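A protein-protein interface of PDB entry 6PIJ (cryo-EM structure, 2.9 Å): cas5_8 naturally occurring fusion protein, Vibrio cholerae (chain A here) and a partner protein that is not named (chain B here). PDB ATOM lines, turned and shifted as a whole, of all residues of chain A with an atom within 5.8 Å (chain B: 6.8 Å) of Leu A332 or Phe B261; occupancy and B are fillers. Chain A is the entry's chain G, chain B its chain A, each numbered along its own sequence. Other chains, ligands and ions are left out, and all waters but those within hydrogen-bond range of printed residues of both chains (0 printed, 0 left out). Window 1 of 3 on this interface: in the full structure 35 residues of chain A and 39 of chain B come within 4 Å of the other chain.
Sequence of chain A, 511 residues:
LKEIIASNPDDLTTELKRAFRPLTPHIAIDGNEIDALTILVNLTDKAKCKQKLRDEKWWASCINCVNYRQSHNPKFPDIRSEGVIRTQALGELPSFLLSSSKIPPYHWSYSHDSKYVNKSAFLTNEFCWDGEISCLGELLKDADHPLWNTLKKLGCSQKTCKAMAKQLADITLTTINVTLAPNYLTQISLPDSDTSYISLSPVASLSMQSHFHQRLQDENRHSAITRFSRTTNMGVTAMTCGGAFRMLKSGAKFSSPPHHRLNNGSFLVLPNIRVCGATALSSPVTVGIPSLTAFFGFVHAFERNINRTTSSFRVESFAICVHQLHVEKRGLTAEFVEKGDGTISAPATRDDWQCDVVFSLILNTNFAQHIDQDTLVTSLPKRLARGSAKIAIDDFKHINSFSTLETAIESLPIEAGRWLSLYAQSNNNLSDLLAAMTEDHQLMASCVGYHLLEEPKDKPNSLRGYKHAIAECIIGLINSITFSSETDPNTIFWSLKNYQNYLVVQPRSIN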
ATOM      1  N   GLY A 277      35.363  18.833 -32.334  1.00  0.00           N
ATOM      2  CA  GLY A 277      34.105  18.295 -32.883  1.00  0.00           C
ATOM      3  C   GLY A 277      33.725  18.938 -34.207  1.00  0.00           C
ATOM      4  O   GLY A 277      32.531  19.260 -34.377  1.00  0.00           O
ATOM      5  N   ARG A 330      31.542   9.794 -32.880  1.00  0.00           N
ATOM      6  CA  ARG A 330      31.143  10.337 -31.551  1.00  0.00           C
ATOM      7  C   ARG A 330      29.620  10.290 -31.394  1.00  0.00           C
ATOM      8  O   ARG A 330      29.163   9.992 -30.278  1.00  0.00           O
ATOM      9  CB  ARG A 330      31.663  11.764 -31.349  1.00  0.00           C
ATOM     10  CG  ARG A 330      32.967  11.821 -30.568  1.00  0.00           C
ATOM     11  CD  ARG A 330      33.440  13.232 -30.302  1.00  0.00           C
ATOM     12  NE  ARG A 330      34.827  13.198 -29.854  1.00  0.00           N
ATOM     13  CZ  ARG A 330      35.730  14.163 -30.016  1.00  0.00           C
ATOM     14  NH1 ARG A 330      35.428  15.296 -30.636  1.00  0.00           N
ATOM     15  NH2 ARG A 330      36.955  13.981 -29.554  1.00  0.00           N
ATOM     16  N   GLY A 331      28.866  10.597 -32.454  1.00  0.00           N
ATOM     17  CA  GLY A 331      27.399  10.722 -32.388  1.00  0.00           C
ATOM     18  C   GLY A 331      26.992  12.061 -31.797  1.00  0.00           C
ATOM     19  O   GLY A 331      27.663  12.525 -30.852  1.00  0.00           O
ATOM     20  N   LEU A 332      25.924  12.659 -32.331  1.00  0.00           N
ATOM     21  CA  LEU A 332      25.476  14.042 -32.018  1.00  0.00           C
ATOM     22  C   LEU A 332      24.069  13.991 -31.411  1.00  0.00           C
ATOM     23  O   LEU A 332      23.189  13.349 -32.017  1.00  0.00           O
ATOM     24  CB  LEU A 332      25.500  14.853 -33.318  1.00  0.00           C
ATOM     25  CG  LEU A 332      25.112  16.327 -33.210  1.00  0.00           C
ATOM     26  CD1 LEU A 332      26.169  17.117 -32.452  1.00  0.00           C
ATOM     27  CD2 LEU A 332      24.896  16.919 -34.594  1.00  0.00           C
ATOM     28  N   THR A 333      23.878  14.645 -30.260  1.00  0.00           N
ATOM     29  CA  THR A 333      22.578  14.752 -29.545  1.00  0.00           C
ATOM     30  C   THR A 333      21.771  15.906 -30.151  1.00  0.00           C
ATOM     31  O   THR A 333      22.237  17.054 -30.060  1.00  0.00           O
ATOM     32  CB  THR A 333      22.783  14.939 -28.035  1.00  0.00           C
ATOM     33  OG1 THR A 333      23.333  13.722 -27.530  1.00  0.00           O
ATOM     34  CG2 THR A 333      21.508  15.264 -27.285  1.00  0.00           C
ATOM     35  N   ALA A 334      20.616  15.599 -30.749  1.00  0.00           N
ATOM     36  CA  ALA A 334      19.603  16.587 -31.190  1.00  0.00           C
ATOM     37  C   ALA A 334      18.777  17.026 -29.974  1.00  0.00           C
ATOM     38  O   ALA A 334      18.712  16.255 -28.994  1.00  0.00           O
ATOM     39  CB  ALA A 334      18.739  16.001 -32.278  1.00  0.00           C
ATOM     40  N   ARG A 350      20.803   9.303 -35.991  1.00  0.00           N
ATOM     41  CA  ARG A 350      21.764   9.026 -37.093  1.00  0.00           C
ATOM     42  C   ARG A 350      23.195   9.265 -36.601  1.00  0.00           C
ATOM     43  O   ARG A 350      23.403  10.218 -35.821  1.00  0.00           O
ATOM     44  CB  ARG A 350      21.447   9.886 -38.321  1.00  0.00           C
ATOM     45  CG  ARG A 350      21.487  11.389 -38.080  1.00  0.00           C
ATOM     46  CD  ARG A 350      20.877  12.149 -39.240  1.00  0.00           C
ATOM     47  NE  ARG A 350      21.011  13.595 -39.104  1.00  0.00           N
ATOM     48  CZ  ARG A 350      22.123  14.300 -39.329  1.00  0.00           C
ATOM     49  NH1 ARG A 350      23.246  13.706 -39.705  1.00  0.00           N
ATOM     50  NH2 ARG A 350      22.106  15.613 -39.170  1.00  0.00           N
ATOM     51  N   ASP A 352      27.187  10.370 -36.766  1.00  0.00           N
ATOM     52  CA  ASP A 352      28.079  11.380 -37.396  1.00  0.00           C
ATOM     53  C   ASP A 352      29.502  11.198 -36.850  1.00  0.00           C
ATOM     54  O   ASP A 352      29.653  10.942 -35.632  1.00  0.00           O
ATOM     55  CB  ASP A 352      27.550  12.805 -37.208  1.00  0.00           C
ATOM     56  CG  ASP A 352      27.688  13.353 -35.797  1.00  0.00           C
ATOM     57  OD1 ASP A 352      27.300  12.639 -34.859  1.00  0.00           O
ATOM     58  OD2 ASP A 352      28.190  14.487 -35.652  1.00  0.00           O
ATOM     59  N   GLN A 354      33.237  12.899 -36.074  1.00  0.00           N
ATOM     60  CA  GLN A 354      33.808  14.206 -35.654  1.00  0.00           C
ATOM     61  C   GLN A 354      35.331  14.070 -35.548  1.00  0.00           C
ATOM     62  O   GLN A 354      35.790  13.097 -34.914  1.00  0.00           O
ATOM     63  CB  GLN A 354      33.192  14.660 -34.330  1.00  0.00           C
ATOM     64  CG  GLN A 354      31.689  14.893 -34.407  1.00  0.00           C
ATOM     65  CD  GLN A 354      31.108  15.436 -33.123  1.00  0.00           C
ATOM     66  OE1 GLN A 354      31.769  16.139 -32.361  1.00  0.00           O
ATOM     67  NE2 GLN A 354      29.849  15.116 -32.876  1.00  0.00           N
ATOM     68  N   ARG A 386      32.277  22.615 -38.093  1.00  0.00           N
ATOM     69  CA  ARG A 386      31.219  22.803 -37.055  1.00  0.00           C
ATOM     70  C   ARG A 386      31.788  22.978 -35.636  1.00  0.00           C
ATOM     71  O   ARG A 386      30.998  23.388 -34.760  1.00  0.00           O
ATOM     72  CB  ARG A 386      30.254  21.614 -37.057  1.00  0.00           C
ATOM     73  CG  ARG A 386      29.218  21.644 -38.171  1.00  0.00           C
ATOM     74  CD  ARG A 386      28.003  20.799 -37.837  1.00  0.00           C
ATOM     75  NE  ARG A 386      27.457  20.156 -39.028  1.00  0.00           N
ATOM     76  CZ  ARG A 386      27.237  18.849 -39.201  1.00  0.00           C
ATOM     77  NH1 ARG A 386      27.487  17.967 -38.244  1.00  0.00           N
ATOM     78  NH2 ARG A 386      26.741  18.424 -40.353  1.00  0.00           N
ATOM     79  N   ARG B  10      25.547  31.196 -31.013  1.00  0.00           N
ATOM     80  CA  ARG B  10      25.741  31.150 -29.538  1.00  0.00           C
ATOM     81  C   ARG B  10      26.857  32.128 -29.145  1.00  0.00           C
ATOM     82  O   ARG B  10      27.828  32.273 -29.918  1.00  0.00           O
ATOM     83  CB  ARG B  10      26.055  29.726 -29.065  1.00  0.00           C
ATOM     84  CG  ARG B  10      27.418  29.205 -29.495  1.00  0.00           C
ATOM     85  CD  ARG B  10      27.614  27.740 -29.165  1.00  0.00           C
ATOM     86  NE  ARG B  10      28.813  27.223 -29.817  1.00  0.00           N
ATOM     87  CZ  ARG B  10      29.551  26.192 -29.401  1.00  0.00           C
ATOM     88  NH1 ARG B  10      29.244  25.522 -28.298  1.00  0.00           N
ATOM     89  NH2 ARG B  10      30.617  25.834 -30.098  1.00  0.00           N
ATOM     90  N   PRO B  14      32.440  27.200 -25.305  1.00  0.00           N
ATOM     91  CA  PRO B  14      33.424  26.342 -24.650  1.00  0.00           C
ATOM     92  C   PRO B  14      33.731  25.120 -25.523  1.00  0.00           C
ATOM     93  O   PRO B  14      32.899  24.775 -26.348  1.00  0.00           O
ATOM     94  CB  PRO B  14      32.692  25.927 -23.371  1.00  0.00           C
ATOM     95  CG  PRO B  14      31.248  25.815 -23.809  1.00  0.00           C
ATOM     96  CD  PRO B  14      31.068  26.840 -24.913  1.00  0.00           C
ATOM     97  N   SER B  15      34.896  24.500 -25.329  1.00  0.00           N
ATOM     98  CA  SER B  15      35.270  23.238 -26.017  1.00  0.00           C
ATOM     99  C   SER B  15      36.366  22.491 -25.245  1.00  0.00           C
ATOM    100  O   SER B  15      37.544  22.891 -25.347  1.00  0.00           O
ATOM    101  CB  SER B  15      35.651  23.500 -27.452  1.00  0.00           C
ATOM    102  OG  SER B  15      36.945  24.075 -27.555  1.00  0.00           O
ATOM    103  N   ASP B  16      35.936  21.513 -24.436  1.00  0.00           N
ATOM    104  CA  ASP B  16      36.667  20.292 -23.987  1.00  0.00           C
ATOM    105  C   ASP B  16      36.974  20.338 -22.488  1.00  0.00           C
ATOM    106  O   ASP B  16      37.021  21.439 -21.912  1.00  0.00           O
ATOM    107  CB  ASP B  16      37.973  20.013 -24.743  1.00  0.00           C
ATOM    108  CG  ASP B  16      37.792  19.298 -26.073  1.00  0.00           C
ATOM    109  OD1 ASP B  16      36.637  18.983 -26.429  1.00  0.00           O
ATOM    110  OD2 ASP B  16      38.811  19.059 -26.747  1.00  0.00           O
ATOM    111  N   TRP B 142      30.935  17.566 -13.976  1.00  0.00           N
ATOM    112  CA  TRP B 142      29.663  16.804 -14.125  1.00  0.00           C
ATOM    113  C   TRP B 142      29.460  15.849 -12.943  1.00  0.00           C
ATOM    114  O   TRP B 142      28.551  16.125 -12.132  1.00  0.00           O
ATOM    115  CB  TRP B 142      29.567  16.111 -15.494  1.00  0.00           C
ATOM    116  CG  TRP B 142      29.058  17.033 -16.559  1.00  0.00           C
ATOM    117  CD1 TRP B 142      29.789  17.723 -17.481  1.00  0.00           C
ATOM    118  CD2 TRP B 142      27.687  17.409 -16.770  1.00  0.00           C
ATOM    119  NE1 TRP B 142      28.965  18.489 -18.261  1.00  0.00           N
ATOM    120  CE2 TRP B 142      27.668  18.314 -17.853  1.00  0.00           C
ATOM    121  CE3 TRP B 142      26.477  17.058 -16.158  1.00  0.00           C
ATOM    122  CZ2 TRP B 142      26.480  18.871 -18.330  1.00  0.00           C
ATOM    123  CZ3 TRP B 142      25.306  17.608 -16.631  1.00  0.00           C
ATOM    124  CH2 TRP B 142      25.310  18.503 -17.703  1.00  0.00           C
ATOM    125  N   PHE B 226      27.297   8.222 -28.936  1.00  0.00           N
ATOM    126  CA  PHE B 226      25.888   7.872 -29.263  1.00  0.00           C
ATOM    127  C   PHE B 226      25.870   6.544 -30.032  1.00  0.00           C
ATOM    128  O   PHE B 226      25.350   5.554 -29.488  1.00  0.00           O
ATOM    129  CB  PHE B 226      25.204   9.011 -30.028  1.00  0.00           C
ATOM    130  CG  PHE B 226      23.719   9.109 -29.800  1.00  0.00           C
ATOM    131  CD1 PHE B 226      22.851   8.193 -30.377  1.00  0.00           C
ATOM    132  CD2 PHE B 226      23.184  10.115 -29.006  1.00  0.00           C
ATOM    133  CE1 PHE B 226      21.483   8.281 -30.168  1.00  0.00           C
ATOM    134  CE2 PHE B 226      21.815  10.202 -28.800  1.00  0.00           C
ATOM    135  CZ  PHE B 226      20.967   9.286 -29.380  1.00  0.00           C
ATOM    136  N   THR B 227      26.447   6.526 -31.240  1.00  0.00           N
ATOM    137  CA  THR B 227      26.627   5.335 -32.119  1.00  0.00           C
ATOM    138  C   THR B 227      25.315   4.549 -32.263  1.00  0.00           C
ATOM    139  O   THR B 227      25.164   3.518 -31.575  1.00  0.00           O
ATOM    140  CB  THR B 227      27.774   4.446 -31.620  1.00  0.00           C
ATOM    141  OG1 THR B 227      27.474   3.948 -30.315  1.00  0.00           O
ATOM    142  CG2 THR B 227      29.092   5.184 -31.590  1.00  0.00           C
ATOM    143  N   GLN B 246      34.048   8.978 -25.485  1.00  0.00           N
ATOM    144  CA  GLN B 246      34.544  10.018 -26.425  1.00  0.00           C
ATOM    145  C   GLN B 246      35.996  10.318 -26.043  1.00  0.00           C
ATOM    146  O   GLN B 246      36.229  10.635 -24.860  1.00  0.00           O
ATOM    147  CB  GLN B 246      33.708  11.300 -26.348  1.00  0.00           C
ATOM    148  CG  GLN B 246      32.220  11.091 -26.596  1.00  0.00           C
ATOM    149  CD  GLN B 246      31.440  12.384 -26.632  1.00  0.00           C
ATOM    150  OE1 GLN B 246      31.998  13.478 -26.647  1.00  0.00           O
ATOM    151  NE2 GLN B 246      30.122  12.264 -26.651  1.00  0.00           N
ATOM    152  N   LEU B 258      35.472  14.198 -21.939  1.00  0.00           N
ATOM    153  CA  LEU B 258      34.272  14.772 -21.259  1.00  0.00           C
ATOM    154  C   LEU B 258      33.614  15.832 -22.158  1.00  0.00           C
ATOM    155  O   LEU B 258      33.376  16.962 -21.688  1.00  0.00           O
ATOM    156  CB  LEU B 258      34.698  15.326 -19.892  1.00  0.00           C
ATOM    157  CG  LEU B 258      33.594  15.836 -18.961  1.00  0.00           C
ATOM    158  CD1 LEU B 258      32.484  14.809 -18.794  1.00  0.00           C
ATOM    159  CD2 LEU B 258      34.170  16.218 -17.604  1.00  0.00           C
ATOM    160  N   GLY B 259      33.362  15.471 -23.422  1.00  0.00           N
ATOM    161  CA  GLY B 259      32.531  16.218 -24.389  1.00  0.00           C
ATOM    162  C   GLY B 259      33.054  17.610 -24.701  1.00  0.00           C
ATOM    163  O   GLY B 259      34.152  17.961 -24.234  1.00  0.00           O
ATOM    164  N   ALA B 260      32.297  18.350 -25.517  1.00  0.00           N
ATOM    165  CA  ALA B 260      32.441  19.804 -25.779  1.00  0.00           C
ATOM    166  C   ALA B 260      31.077  20.492 -25.621  1.00  0.00           C
ATOM    167  O   ALA B 260      31.026  21.554 -24.971  1.00  0.00           O
ATOM    168  CB  ALA B 260      33.019  20.030 -27.154  1.00  0.00           C
ATOM    169  N   PHE B 261      30.023  19.911 -26.206  1.00  0.00           N
ATOM    170  CA  PHE B 261      28.602  20.318 -26.033  1.00  0.00           C
ATOM    171  C   PHE B 261      28.141  20.021 -24.601  1.00  0.00           C
ATOM    172  O   PHE B 261      27.336  20.814 -24.070  1.00  0.00           O
ATOM    173  CB  PHE B 261      27.703  19.612 -27.050  1.00  0.00           C
ATOM    174  CG  PHE B 261      28.010  19.957 -28.485  1.00  0.00           C
ATOM    175  CD1 PHE B 261      27.755  21.230 -28.975  1.00  0.00           C
ATOM    176  CD2 PHE B 261      28.565  19.018 -29.342  1.00  0.00           C
ATOM    177  CE1 PHE B 261      28.045  21.555 -30.292  1.00  0.00           C
ATOM    178  CE2 PHE B 261      28.850  19.343 -30.661  1.00  0.00           C
ATOM    179  CZ  PHE B 261      28.589  20.610 -31.134  1.00  0.00           C
ATOM    180  N   LYS B 262      28.620  18.919 -24.007  1.00  0.00           N
ATOM    181  CA  LYS B 262      28.312  18.529 -22.603  1.00  0.00           C
ATOM    182  C   LYS B 262      28.803  19.637 -21.663  1.00  0.00           C
ATOM    183  O   LYS B 262      28.010  20.075 -20.818  1.00  0.00           O
ATOM    184  CB  LYS B 262      28.929  17.173 -22.243  1.00  0.00           C
ATOM    185  CG  LYS B 262      28.423  16.577 -20.935  1.00  0.00           C
ATOM    186  CD  LYS B 262      28.618  15.083 -20.806  1.00  0.00           C
ATOM    187  CE  LYS B 262      28.070  14.526 -19.507  1.00  0.00           C
ATOM    188  NZ  LYS B 262      26.592  14.616 -19.439  1.00  0.00           N
ATOM    189  N   THR B 263      30.051  20.089 -21.831  1.00  0.00           N
ATOM    190  CA  THR B 263      30.656  21.226 -21.082  1.00  0.00           C
ATOM    191  C   THR B 263      29.768  22.469 -21.237  1.00  0.00           C
ATOM    192  O   THR B 263      29.415  23.070 -20.204  1.00  0.00           O
ATOM    193  CB  THR B 263      32.091  21.506 -21.550  1.00  0.00           C
ATOM    194  OG1 THR B 263      32.808  20.271 -21.571  1.00  0.00           O
ATOM    195  CG2 THR B 263      32.814  22.498 -20.666  1.00  0.00           C
ATOM    196  N   GLY B 264      29.407  22.812 -22.479  1.00  0.00           N
ATOM    197  CA  GLY B 264      28.502  23.929 -22.820  1.00  0.00           C
ATOM    198  C   GLY B 264      27.154  23.815 -22.128  1.00  0.00           C
ATOM    199  O   GLY B 264      26.634  24.858 -21.685  1.00  0.00           O
ATOM    200  N   ALA B 265      26.611  22.597 -22.036  1.00  0.00           N
ATOM    201  CA  ALA B 265      25.338  22.280 -21.343  1.00  0.00           C
ATOM    202  C   ALA B 265      25.473  22.524 -19.832  1.00  0.00           C
ATOM    203  O   ALA B 265      24.460  22.903 -19.215  1.00  0.00           O
ATOM    204  CB  ALA B 265      24.916  20.860 -21.638  1.00  0.00           C
ATOM    205  N   ALA B 266      26.669  22.318 -19.263  1.00  0.00           N
ATOM    206  CA  ALA B 266      26.969  22.507 -17.822  1.00  0.00           C
ATOM    207  C   ALA B 266      26.929  23.997 -17.457  1.00  0.00           C
ATOM    208  O   ALA B 266      26.376  24.320 -16.387  1.00  0.00           O
ATOM    209  CB  ALA B 266      28.308  21.903 -17.470  1.00  0.00           C
ATOM    210  N   ARG B 282      18.908  23.235 -17.704  1.00  0.00           N
ATOM    211  CA  ARG B 282      19.597  23.547 -18.985  1.00  0.00           C
ATOM    212  C   ARG B 282      18.730  24.556 -19.744  1.00  0.00           C
ATOM    213  O   ARG B 282      17.593  24.184 -20.102  1.00  0.00           O
ATOM    214  CB  ARG B 282      19.798  22.257 -19.790  1.00  0.00           C
ATOM    215  CG  ARG B 282      20.241  22.448 -21.235  1.00  0.00           C
ATOM    216  CD  ARG B 282      21.744  22.523 -21.386  1.00  0.00           C
ATOM    217  NE  ARG B 282      22.138  22.673 -22.781  1.00  0.00           N
ATOM    218  CZ  ARG B 282      22.237  23.826 -23.449  1.00  0.00           C
ATOM    219  NH1 ARG B 282      21.971  24.985 -22.866  1.00  0.00           N
ATOM    220  NH2 ARG B 282      22.609  23.809 -24.719  1.00  0.00           N
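Printed residues of chain B that touch a printed residue of chain A: Phe B226, Gln B246 and Phe B261. Hydrophobic or aromatic side chains of chain B that line the printed part of chain A: Phe B226 and Phe B261. Among the printed residues, no Asp or Glu carboxylate lies within 4 Å of a Lys or Arg side-chain nitrogen of the other chain.
OD1 of Asp A352 is in hydrogen-bond range of N of Leu A332 (2.9 Å). O of Asp A352 is in hydrogen-bond range of N of Gly A331 (3.3 Å).
Among the printed residues, merely in contact across the chains: Arg A330 with Gln B246 (3.9 Å), Gly A331 with Phe B226 (3.6 Å), Leu A332 with Phe B261 (3.9 Å) and Thr A333 with Phe B226 (3.9 Å).
The backbone NH of Phe B226 sits at hydrogen-bond distance from the backbone carbonyl oxygen of Arg A330 (2.9 Å).
Leu A332 touches just one residue of chain B: Phe B261 (3.9 Å). Of the printed residues of chain A, Phe B261 touches Leu A332 (3.9 Å). Of the printed residues of chain B, Arg A330 touches Phe B226 (2.9 Å) and Gln B246 (3.9 Å). Of the printed residues of chain B, Gly A331 touches Phe B226 (3.6 Å). The nearest residue of chain B that does not touch Leu A332 is Phe B226 (4.4 Å).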
